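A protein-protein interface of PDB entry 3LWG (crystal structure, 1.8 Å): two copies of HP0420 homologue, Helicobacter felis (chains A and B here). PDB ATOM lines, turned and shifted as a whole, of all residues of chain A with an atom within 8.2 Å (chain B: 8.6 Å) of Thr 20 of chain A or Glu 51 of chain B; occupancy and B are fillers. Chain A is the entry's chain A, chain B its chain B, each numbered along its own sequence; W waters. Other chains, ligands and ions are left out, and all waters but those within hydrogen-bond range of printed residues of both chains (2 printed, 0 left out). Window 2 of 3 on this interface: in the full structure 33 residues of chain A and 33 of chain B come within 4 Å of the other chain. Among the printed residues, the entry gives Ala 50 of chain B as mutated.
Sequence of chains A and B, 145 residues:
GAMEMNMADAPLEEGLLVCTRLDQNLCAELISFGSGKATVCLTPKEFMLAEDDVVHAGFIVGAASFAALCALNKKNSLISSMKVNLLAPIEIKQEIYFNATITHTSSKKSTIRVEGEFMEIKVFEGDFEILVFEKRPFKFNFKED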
ATOM      1  N   LEU A  16     -32.346 -21.444 -31.914  1.00  0.00           N
ATOM      2  CA  LEU A  16     -31.498 -21.132 -30.758  1.00  0.00           C
ATOM      3  C   LEU A  16     -31.486 -19.632 -30.414  1.00  0.00           C
ATOM      4  O   LEU A  16     -31.140 -18.805 -31.260  1.00  0.00           O
ATOM      5  CB  LEU A  16     -30.092 -21.567 -31.103  1.00  0.00           C
ATOM      6  CG  LEU A  16     -29.088 -21.601 -29.962  1.00  0.00           C
ATOM      7  CD1 LEU A  16     -29.514 -22.676 -28.959  1.00  0.00           C
ATOM      8  CD2 LEU A  16     -27.716 -21.929 -30.576  1.00  0.00           C
ATOM      9  N   LEU A  17     -31.868 -19.281 -29.197  1.00  0.00           N
ATOM     10  CA  LEU A  17     -31.982 -17.879 -28.803  1.00  0.00           C
ATOM     11  C   LEU A  17     -30.730 -17.348 -28.100  1.00  0.00           C
ATOM     12  O   LEU A  17     -30.666 -16.161 -27.713  1.00  0.00           O
ATOM     13  CB  LEU A  17     -33.197 -17.697 -27.913  1.00  0.00           C
ATOM     14  CG  LEU A  17     -34.444 -18.342 -28.551  1.00  0.00           C
ATOM     15  CD1 LEU A  17     -35.694 -18.331 -27.651  1.00  0.00           C
ATOM     16  CD2 LEU A  17     -34.709 -17.665 -29.899  1.00  0.00           C
ATOM     17  N   VAL A  18     -29.748 -18.227 -27.944  1.00  0.00           N
ATOM     18  CA  VAL A  18     -28.638 -17.963 -27.049  1.00  0.00           C
ATOM     19  C   VAL A  18     -27.263 -18.130 -27.692  1.00  0.00           C
ATOM     20  O   VAL A  18     -27.098 -18.708 -28.779  1.00  0.00           O
ATOM     21  CB  VAL A  18     -28.669 -18.885 -25.804  1.00  0.00           C
ATOM     22  CG1 VAL A  18     -29.948 -18.697 -25.056  1.00  0.00           C
ATOM     23  CG2 VAL A  18     -28.426 -20.362 -26.220  1.00  0.00           C
ATOM     24  N   CYS A  19     -26.273 -17.621 -26.979  1.00  0.00           N
ATOM     25  CA  CYS A  19     -24.891 -17.682 -27.431  1.00  0.00           C
ATOM     26  C   CYS A  19     -24.687 -17.184 -28.852  1.00  0.00           C
ATOM     27  O   CYS A  19     -23.926 -17.766 -29.602  1.00  0.00           O
ATOM     28  CB  CYS A  19     -24.367 -19.115 -27.267  1.00  0.00           C
ATOM     29  SG  CYS A  19     -24.299 -19.539 -25.470  1.00  0.00           S
ATOM     30  N   THR A  20     -25.306 -16.069 -29.204  1.00  0.00           N
ATOM     31  CA  THR A  20     -25.272 -15.626 -30.584  1.00  0.00           C
ATOM     32  C   THR A  20     -23.874 -15.150 -31.000  1.00  0.00           C
ATOM     33  O   THR A  20     -23.586 -15.069 -32.197  1.00  0.00           O
ATOM     34  CB  THR A  20     -26.325 -14.488 -30.842  1.00  0.00           C
ATOM     35  OG1 THR A  20     -26.056 -13.396 -29.959  1.00  0.00           O
ATOM     36  CG2 THR A  20     -27.715 -14.988 -30.547  1.00  0.00           C
ATOM     37  N   ARG A  21     -22.985 -14.875 -30.037  1.00  0.00           N
ATOM     38  CA  ARG A  21     -21.630 -14.405 -30.397  1.00  0.00           C
ATOM     39  C   ARG A  21     -20.573 -15.459 -30.111  1.00  0.00           C
ATOM     40  O   ARG A  21     -19.374 -15.246 -30.371  1.00  0.00           O
ATOM     41  CB  ARG A  21     -21.257 -13.086 -29.658  1.00  0.00           C
ATOM     42  CG  ARG A  21     -22.101 -11.888 -30.023  1.00  0.00           C
ATOM     43  CD  ARG A  21     -21.865 -11.376 -31.497  1.00  0.00           C
ATOM     44  NE  ARG A  21     -20.480 -10.960 -31.734  1.00  0.00           N
ATOM     45  CZ  ARG A  21     -19.958  -9.763 -31.413  1.00  0.00           C
ATOM     46  NH1 ARG A  21     -20.701  -8.826 -30.839  1.00  0.00           N
ATOM     47  NH2 ARG A  21     -18.671  -9.505 -31.664  1.00  0.00           N
ATOM     48  N   LEU A  22     -20.997 -16.600 -29.576  1.00  0.00           N
ATOM     49  CA  LEU A  22     -20.049 -17.611 -29.151  1.00  0.00           C
ATOM     50  C   LEU A  22     -19.314 -18.268 -30.334  1.00  0.00           C
ATOM     51  O   LEU A  22     -19.924 -18.893 -31.224  1.00  0.00           O
ATOM     52  CB  LEU A  22     -20.783 -18.705 -28.382  1.00  0.00           C
ATOM     53  CG  LEU A  22     -19.829 -19.672 -27.704  1.00  0.00           C
ATOM     54  CD1 LEU A  22     -19.332 -19.059 -26.394  1.00  0.00           C
ATOM     55  CD2 LEU A  22     -20.524 -20.969 -27.404  1.00  0.00           C
ATOM     56  N   ASP A  23     -18.010 -18.199 -30.313  1.00  0.00           N
ATOM     57  CA  ASP A  23     -17.254 -18.915 -31.344  1.00  0.00           C
ATOM     58  C   ASP A  23     -17.123 -20.407 -31.003  1.00  0.00           C
ATOM     59  O   ASP A  23     -16.333 -20.789 -30.144  1.00  0.00           O
ATOM     60  CB  ASP A  23     -15.878 -18.298 -31.522  1.00  0.00           C
ATOM     61  CG  ASP A  23     -15.103 -18.928 -32.672  1.00  0.00           C
ATOM     62  OD1 ASP A  23     -15.637 -19.842 -33.361  1.00  0.00           O
ATOM     63  OD2 ASP A  23     -13.978 -18.468 -32.914  1.00  0.00           O
ATOM     64  N   PHE A  66     -21.925 -23.674 -22.240  1.00  0.00           N
ATOM     65  CA  PHE A  66     -22.586 -23.579 -23.563  1.00  0.00           C
ATOM     66  C   PHE A  66     -23.768 -24.580 -23.601  1.00  0.00           C
ATOM     67  O   PHE A  66     -24.917 -24.204 -23.887  1.00  0.00           O
ATOM     68  CB  PHE A  66     -21.532 -23.867 -24.641  1.00  0.00           C
ATOM     69  CG  PHE A  66     -22.044 -23.826 -26.072  1.00  0.00           C
ATOM     70  CD1 PHE A  66     -23.078 -22.972 -26.481  1.00  0.00           C
ATOM     71  CD2 PHE A  66     -21.407 -24.606 -27.032  1.00  0.00           C
ATOM     72  CE1 PHE A  66     -23.510 -22.960 -27.804  1.00  0.00           C
ATOM     73  CE2 PHE A  66     -21.812 -24.591 -28.401  1.00  0.00           C
ATOM     74  CZ  PHE A  66     -22.860 -23.744 -28.787  1.00  0.00           C
ATOM     75  N   LEU A  69     -26.630 -23.292 -21.241  1.00  0.00           N
ATOM     76  CA  LEU A  69     -27.392 -22.180 -21.795  1.00  0.00           C
ATOM     77  C   LEU A  69     -28.284 -22.668 -22.929  1.00  0.00           C
ATOM     78  O   LEU A  69     -29.406 -22.145 -23.107  1.00  0.00           O
ATOM     79  CB  LEU A  69     -26.467 -21.082 -22.320  1.00  0.00           C
ATOM     80  CG  LEU A  69     -25.758 -20.310 -21.221  1.00  0.00           C
ATOM     81  CD1 LEU A  69     -24.557 -19.509 -21.779  1.00  0.00           C
ATOM     82  CD2 LEU A  69     -26.742 -19.319 -20.504  1.00  0.00           C
ATOM     83  N   LYS A  74     -32.988 -19.429 -23.582  1.00  0.00           N
ATOM     84  CA  LYS A  74     -33.747 -18.209 -23.323  1.00  0.00           C
ATOM     85  C   LYS A  74     -32.924 -16.975 -23.640  1.00  0.00           C
ATOM     86  O   LYS A  74     -31.753 -16.878 -23.290  1.00  0.00           O
ATOM     87  CB  LYS A  74     -34.204 -18.124 -21.857  1.00  0.00           C
ATOM     88  CG  LYS A  74     -35.276 -19.114 -21.531  1.00  0.00           C
ATOM     89  CD  LYS A  74     -36.610 -18.711 -22.082  1.00  0.00           C
ATOM     90  CE  LYS A  74     -37.702 -19.723 -21.634  1.00  0.00           C
ATOM     91  NZ  LYS A  74     -38.984 -19.340 -22.355  1.00  0.00           N
ATOM     92  N   LYS A  75     -33.577 -16.040 -24.317  1.00  0.00           N
ATOM     93  CA  LYS A  75     -32.984 -14.733 -24.585  1.00  0.00           C
ATOM     94  C   LYS A  75     -32.679 -14.015 -23.272  1.00  0.00           C
ATOM     95  O   LYS A  75     -33.404 -14.181 -22.294  1.00  0.00           O
ATOM     96  CB  LYS A  75     -33.985 -13.928 -25.434  1.00  0.00           C
ATOM     97  CG  LYS A  75     -33.634 -12.469 -25.659  1.00  0.00           C
ATOM     98  CD  LYS A  75     -34.393 -11.915 -26.864  1.00  0.00           C
ATOM     99  CE  LYS A  75     -33.921 -10.491 -27.195  1.00  0.00           C
ATOM    100  NZ  LYS A  75     -32.410 -10.398 -27.313  1.00  0.00           N
ATOM    101  N   ASN A  76     -31.591 -13.236 -23.243  1.00  0.00           N
ATOM    102  CA  ASN A  76     -31.248 -12.405 -22.077  1.00  0.00           C
ATOM    103  C   ASN A  76     -30.987 -13.282 -20.894  1.00  0.00           C
ATOM    104  O   ASN A  76     -31.403 -12.944 -19.796  1.00  0.00           O
ATOM    105  CB  ASN A  76     -32.361 -11.398 -21.677  1.00  0.00           C
ATOM    106  CG  ASN A  76     -32.765 -10.447 -22.809  1.00  0.00           C
ATOM    107  OD1 ASN A  76     -31.917  -9.911 -23.510  1.00  0.00           O
ATOM    108  ND2 ASN A  76     -34.078 -10.231 -22.977  1.00  0.00           N
ATOM    109  N   SER A  77     -30.332 -14.416 -21.124  1.00  0.00           N
ATOM    110  CA  SER A  77     -29.919 -15.242 -19.995  1.00  0.00           C
ATOM    111  C   SER A  77     -28.423 -15.095 -19.722  1.00  0.00           C
ATOM    112  O   SER A  77     -27.656 -14.741 -20.637  1.00  0.00           O
ATOM    113  CB  SER A  77     -30.290 -16.707 -20.214  1.00  0.00           C
ATOM    114  OG  SER A  77     -29.673 -17.157 -21.384  1.00  0.00           O
ATOM    115  N   LEU A  78     -28.032 -15.434 -18.481  1.00  0.00           N
ATOM    116  CA  LEU A  78     -26.637 -15.359 -17.999  1.00  0.00           C
ATOM    117  C   LEU A  78     -26.431 -16.459 -16.985  1.00  0.00           C
ATOM    118  O   LEU A  78     -27.274 -16.659 -16.132  1.00  0.00           O
ATOM    119  CB  LEU A  78     -26.415 -14.069 -17.179  1.00  0.00           C
ATOM    120  CG  LEU A  78     -26.641 -12.655 -17.667  1.00  0.00           C
ATOM    121  CD1 LEU A  78     -26.215 -11.637 -16.613  1.00  0.00           C
ATOM    122  CD2 LEU A  78     -25.880 -12.426 -18.976  1.00  0.00           C
ATOM    123  N   LYS B  45     -11.764  -9.961 -24.799  1.00  0.00           N
ATOM    124  CA  LYS B  45     -11.677  -9.689 -26.209  1.00  0.00           C
ATOM    125  C   LYS B  45     -12.945 -10.148 -26.925  1.00  0.00           C
ATOM    126  O   LYS B  45     -13.733 -10.925 -26.367  1.00  0.00           O
ATOM    127  CB  LYS B  45     -10.437 -10.414 -26.814  1.00  0.00           C
ATOM    128  CG  LYS B  45      -9.143 -10.155 -26.041  1.00  0.00           C
ATOM    129  CD  LYS B  45      -8.928  -8.658 -25.859  1.00  0.00           C
ATOM    130  CE  LYS B  45      -7.500  -8.347 -25.365  1.00  0.00           C
ATOM    131  NZ  LYS B  45      -7.191  -8.916 -24.008  1.00  0.00           N
ATOM    132  N   GLU B  46     -13.122  -9.704 -28.174  1.00  0.00           N
ATOM    133  CA  GLU B  46     -14.317 -10.114 -28.943  1.00  0.00           C
ATOM    134  C   GLU B  46     -14.515 -11.613 -29.003  1.00  0.00           C
ATOM    135  O   GLU B  46     -15.649 -12.098 -28.894  1.00  0.00           O
ATOM    136  CB  GLU B  46     -14.253  -9.560 -30.381  1.00  0.00           C
ATOM    137  CG  GLU B  46     -14.040  -8.118 -30.268  1.00  0.00           C
ATOM    138  CD  GLU B  46     -14.199  -7.372 -31.566  1.00  0.00           C
ATOM    139  OE1 GLU B  46     -14.378  -8.042 -32.631  1.00  0.00           O
ATOM    140  OE2 GLU B  46     -14.132  -6.112 -31.486  1.00  0.00           O
ATOM    141  N   MET B  48     -14.093 -13.732 -26.900  1.00  0.00           N
ATOM    142  CA  MET B  48     -14.483 -14.296 -25.581  1.00  0.00           C
ATOM    143  C   MET B  48     -15.985 -14.104 -25.330  1.00  0.00           C
ATOM    144  O   MET B  48     -16.524 -14.518 -24.313  1.00  0.00           O
ATOM    145  CB  MET B  48     -13.721 -13.606 -24.473  1.00  0.00           C
ATOM    146  CG  MET B  48     -12.256 -13.956 -24.488  1.00  0.00           C
ATOM    147  SD  MET B  48     -11.424 -13.140 -23.126  1.00  0.00           S
ATOM    148  CE  MET B  48      -9.798 -13.916 -23.229  1.00  0.00           C
ATOM    149  N   LEU B  49     -16.676 -13.461 -26.256  1.00  0.00           N
ATOM    150  CA  LEU B  49     -18.096 -13.172 -26.022  1.00  0.00           C
ATOM    151  C   LEU B  49     -19.044 -14.378 -26.231  1.00  0.00           C
ATOM    152  O   LEU B  49     -18.902 -15.141 -27.213  1.00  0.00           O
ATOM    153  CB  LEU B  49     -18.574 -12.029 -26.914  1.00  0.00           C
ATOM    154  CG  LEU B  49     -17.973 -10.642 -26.699  1.00  0.00           C
ATOM    155  CD1 LEU B  49     -18.577  -9.685 -27.742  1.00  0.00           C
ATOM    156  CD2 LEU B  49     -18.263 -10.155 -25.247  1.00  0.00           C
ATOM    157  N   ALA B  50     -20.023 -14.517 -25.339  1.00  0.00           N
ATOM    158  CA  ALA B  50     -21.164 -15.430 -25.562  1.00  0.00           C
ATOM    159  C   ALA B  50     -22.301 -14.716 -26.275  1.00  0.00           C
ATOM    160  O   ALA B  50     -22.941 -15.296 -27.195  1.00  0.00           O
ATOM    161  CB  ALA B  50     -21.674 -16.020 -24.214  1.00  0.00           C
ATOM    162  N   GLU B  51     -22.572 -13.494 -25.821  1.00  0.00           N
ATOM    163  CA  GLU B  51     -23.605 -12.576 -26.391  1.00  0.00           C
ATOM    164  C   GLU B  51     -22.936 -11.224 -26.673  1.00  0.00           C
ATOM    165  O   GLU B  51     -21.771 -11.005 -26.309  1.00  0.00           O
ATOM    166  CB  GLU B  51     -24.763 -12.356 -25.385  1.00  0.00           C
ATOM    167  CG  GLU B  51     -25.260 -13.635 -24.731  1.00  0.00           C
ATOM    168  CD  GLU B  51     -26.112 -14.509 -25.652  1.00  0.00           C
ATOM    169  OE1 GLU B  51     -26.327 -14.138 -26.837  1.00  0.00           O
ATOM    170  OE2 GLU B  51     -26.581 -15.570 -25.183  1.00  0.00           O
ATOM    171  N   ASP B  52     -23.659 -10.280 -27.286  1.00  0.00           N
ATOM    172  CA  ASP B  52     -22.978  -9.020 -27.613  1.00  0.00           C
ATOM    173  C   ASP B  52     -22.374  -8.380 -26.363  1.00  0.00           C
ATOM    174  O   ASP B  52     -21.286  -7.806 -26.421  1.00  0.00           O
ATOM    175  CB  ASP B  52     -23.951  -7.995 -28.192  1.00  0.00           C
ATOM    176  CG  ASP B  52     -24.434  -8.350 -29.569  1.00  0.00           C
ATOM    177  OD1 ASP B  52     -25.460  -7.751 -29.948  1.00  0.00           O
ATOM    178  OD2 ASP B  52     -23.820  -9.208 -30.248  1.00  0.00           O
ATOM    179  N   ASP B  53     -23.146  -8.380 -25.273  1.00  0.00           N
ATOM    180  CA  ASP B  53     -22.744  -7.738 -24.019  1.00  0.00           C
ATOM    181  C   ASP B  53     -22.455  -8.696 -22.886  1.00  0.00           C
ATOM    182  O   ASP B  53     -22.592  -8.302 -21.703  1.00  0.00           O
ATOM    183  CB  ASP B  53     -23.844  -6.809 -23.525  1.00  0.00           C
ATOM    184  CG  ASP B  53     -24.227  -5.799 -24.565  1.00  0.00           C
ATOM    185  OD1 ASP B  53     -23.417  -5.617 -25.507  1.00  0.00           O
ATOM    186  OD2 ASP B  53     -25.323  -5.206 -24.449  1.00  0.00           O
ATOM    187  N   VAL B  54     -22.085  -9.941 -23.212  1.00  0.00           N
ATOM    188  CA  VAL B  54     -21.864 -10.922 -22.151  1.00  0.00           C
ATOM    189  C   VAL B  54     -20.655 -11.787 -22.482  1.00  0.00           C
ATOM    190  O   VAL B  54     -20.675 -12.539 -23.456  1.00  0.00           O
ATOM    191  CB  VAL B  54     -23.085 -11.834 -21.915  1.00  0.00           C
ATOM    192  CG1 VAL B  54     -22.747 -12.854 -20.768  1.00  0.00           C
ATOM    193  CG2 VAL B  54     -24.349 -11.002 -21.548  1.00  0.00           C
ATOM    194  N   VAL B  55     -19.598 -11.674 -21.661  1.00  0.00           N
ATOM    195  CA  VAL B  55     -18.418 -12.550 -21.817  1.00  0.00           C
ATOM    196  C   VAL B  55     -18.776 -13.948 -21.354  1.00  0.00           C
ATOM    197  O   VAL B  55     -19.421 -14.120 -20.295  1.00  0.00           O
ATOM    198  CB  VAL B  55     -17.221 -12.005 -21.006  1.00  0.00           C
ATOM    199  CG1 VAL B  55     -16.028 -13.023 -20.954  1.00  0.00           C
ATOM    200  CG2 VAL B  55     -16.753 -10.671 -21.643  1.00  0.00           C
ATOM    201  N   HIS B  56     -18.323 -14.943 -22.123  1.00  0.00           N
ATOM    202  CA  HIS B  56     -18.697 -16.313 -21.886  1.00  0.00           C
ATOM    203  C   HIS B  56     -18.120 -16.774 -20.550  1.00  0.00           C
ATOM    204  O   HIS B  56     -16.966 -16.399 -20.174  1.00  0.00           O
ATOM    205  CB  HIS B  56     -18.101 -17.192 -22.990  1.00  0.00           C
ATOM    206  CG  HIS B  56     -18.600 -18.590 -22.918  1.00  0.00           C
ATOM    207  ND1 HIS B  56     -17.783 -19.702 -23.031  1.00  0.00           N
ATOM    208  CD2 HIS B  56     -19.846 -19.051 -22.772  1.00  0.00           C
ATOM    209  CE1 HIS B  56     -18.521 -20.789 -22.954  1.00  0.00           C
ATOM    210  NE2 HIS B  56     -19.773 -20.423 -22.780  1.00  0.00           N
ATOM    211  N   ALA B  57     -18.923 -17.539 -19.803  1.00  0.00           N
ATOM    212  CA  ALA B  57     -18.471 -17.962 -18.460  1.00  0.00           C
ATOM    213  C   ALA B  57     -17.185 -18.746 -18.499  1.00  0.00           C
ATOM    214  O   ALA B  57     -16.442 -18.752 -17.513  1.00  0.00           O
ATOM    215  CB  ALA B  57     -19.580 -18.815 -17.703  1.00  0.00           C
ATOM    216  N   ILE B  90     -19.961  -9.347 -17.716  1.00  0.00           N
ATOM    217  CA  ILE B  90     -18.794  -8.581 -18.055  1.00  0.00           C
ATOM    218  C   ILE B  90     -18.855  -8.335 -19.531  1.00  0.00           C
ATOM    219  O   ILE B  90     -19.281  -9.204 -20.288  1.00  0.00           O
ATOM    220  CB  ILE B  90     -17.513  -9.365 -17.693  1.00  0.00           C
ATOM    221  CG1 ILE B  90     -17.580  -9.735 -16.222  1.00  0.00           C
ATOM    222  CG2 ILE B  90     -16.219  -8.566 -18.078  1.00  0.00           C
ATOM    223  CD1 ILE B  90     -17.608  -8.564 -15.350  1.00  0.00           C
ATOM    224  N   GLU B  91     -18.428  -7.146 -19.920  1.00  0.00           N
ATOM    225  CA  GLU B  91     -18.358  -6.759 -21.315  1.00  0.00           C
ATOM    226  C   GLU B  91     -16.941  -6.645 -21.828  1.00  0.00           C
ATOM    227  O   GLU B  91     -16.006  -6.468 -21.041  1.00  0.00           O
ATOM    228  CB  GLU B  91     -19.040  -5.390 -21.448  1.00  0.00           C
ATOM    229  CG  GLU B  91     -20.570  -5.488 -21.126  1.00  0.00           C
ATOM    230  CD  GLU B  91     -21.183  -4.104 -21.200  1.00  0.00           C
ATOM    231  OE1 GLU B  91     -21.626  -3.629 -20.167  1.00  0.00           O
ATOM    232  OE2 GLU B  91     -21.190  -3.507 -22.289  1.00  0.00           O
ATOM    233  N   ILE B  92     -16.778  -6.632 -23.153  1.00  0.00           N
ATOM    234  CA  ILE B  92     -15.450  -6.365 -23.693  1.00  0.00           C
ATOM    235  C   ILE B  92     -14.883  -5.066 -23.156  1.00  0.00           C
ATOM    236  O   ILE B  92     -15.621  -4.129 -22.869  1.00  0.00           O
ATOM    237  CB  ILE B  92     -15.436  -6.253 -25.237  1.00  0.00           C
ATOM    238  CG1 ILE B  92     -16.528  -5.282 -25.689  1.00  0.00           C
ATOM    239  CG2 ILE B  92     -15.590  -7.628 -25.827  1.00  0.00           C
ATOM    240  CD1 ILE B  92     -16.044  -3.778 -25.790  1.00  0.00           C
HETATM  241  O   HOH W   1     -26.247 -11.008 -28.258  1.00  0.00           O
HETATM  242  O   HOH W   2     -16.753 -16.930 -27.936  1.00  0.00           O
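Thr 20 of chain A touches two residues of chain B. Of chain A, only Val 18, Cys 19, Thr 20 and Arg 21 come within 4 Å of Glu 51 of chain B. Ala 50 of chain B touches just these residues of chain A: Cys 19 (3.1 Å), Thr 20 (3.2 Å), Arg 21 (2.9 Å) and Leu 22 (3.3 Å). Printed residues of chain A within 4 Å of His 56 of chain B: Leu 22 and Phe 66. Of the printed residues of chain A, Leu 49 of chain B touches Arg 21 and Leu 22. Of the printed residues of chain B, Cys 19 of chain A touches Ala 50 and Glu 51. Printed residues of chain B within 4 Å of Arg 21 of chain A: Leu 49, Ala 50, Glu 51 and Asp 52. The nearest residue of chain A that does not touch Glu 51 of chain B is Ser 77 of chain A (4.7 Å).
Water W1 lies within hydrogen-bond range of the backbone NH of Asp 52 of chain B (2.9 Å), the side-chain hydroxyl of Thr 20 of chain A (2.9 Å) and the side-chain carboxylate of Glu 51 of chain B (3.4 Å). Water W2 lies within hydrogen-bond range of O of Leu 49 of chain B and N of Asp 23 of chain A.
The backbone carbonyl oxygen (O) of Met 48 of chain B is in hydrogen-bond range of the backbone NH (N) of His 56 of chain B (2.9 Å).
No position is printed for both chains.
Val 18 of chain A touches Glu 51 of chain B. Ala 50 of chain B touches Cys 19 of chain A (O to C, 3.1 Å). Glu 51 of chain B touches Arg 21 of chain A (C to CG, 3.5 Å). Leu 22 of chain A touches His 56 of chain B. Phe 66 of chain A touches His 56 of chain B (N to NE2, 3.9 Å). Val 54 of chain B touches Leu 78 of chain A.
The backbone NH of Cys 19 of chain A sits at hydrogen-bond distance from the side-chain carboxylate of Glu 51 of chain B, at 2.7 Å. N of Thr 20 of chain A is in hydrogen-bond range of O of Ala 50 of chain B, 3.2 Å away. OG1 of Thr 20 of chain A is in hydrogen-bond range of OE1 of Glu 51 of chain B. N of Arg 21 of chain A lies within hydrogen-bond range of O of Ala 50 of chain B (2.9 Å). The guanidinium group of Arg 21 of chain A is in salt-bridge range of the side-chain carboxylate of Asp 52 of chain B (3.2 Å). N of Leu 22 of chain A lies close to O of Leu 49 of chain B (3.5 Å). N of Leu 22 of chain A is in hydrogen-bond range of O of Ala 50 of chain B (3.3 Å). The backbone carbonyl oxygen (O) of Leu 49 of chain B lies close to the backbone carbonyl oxygen (O) of Arg 21 of chain A, at 3.2 Å.
Printed residues of chain A that touch a printed residue of chain B: Val 18, Cys 19, Thr 20, Arg 21, Leu 22, Phe 66 and Leu 78. Of the 15 printed residues of chain B, 6 touch a printed residue of chain A. Hydrophobic or aromatic side chains of chain B within 4 Å of the printed part of chain A: Leu 49, Val 54 and His 56. Along chain B the printed residues that touch a printed residue of chain A span positions 49 to 56. Among the printed residues, 14 pairs touch across the chains.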
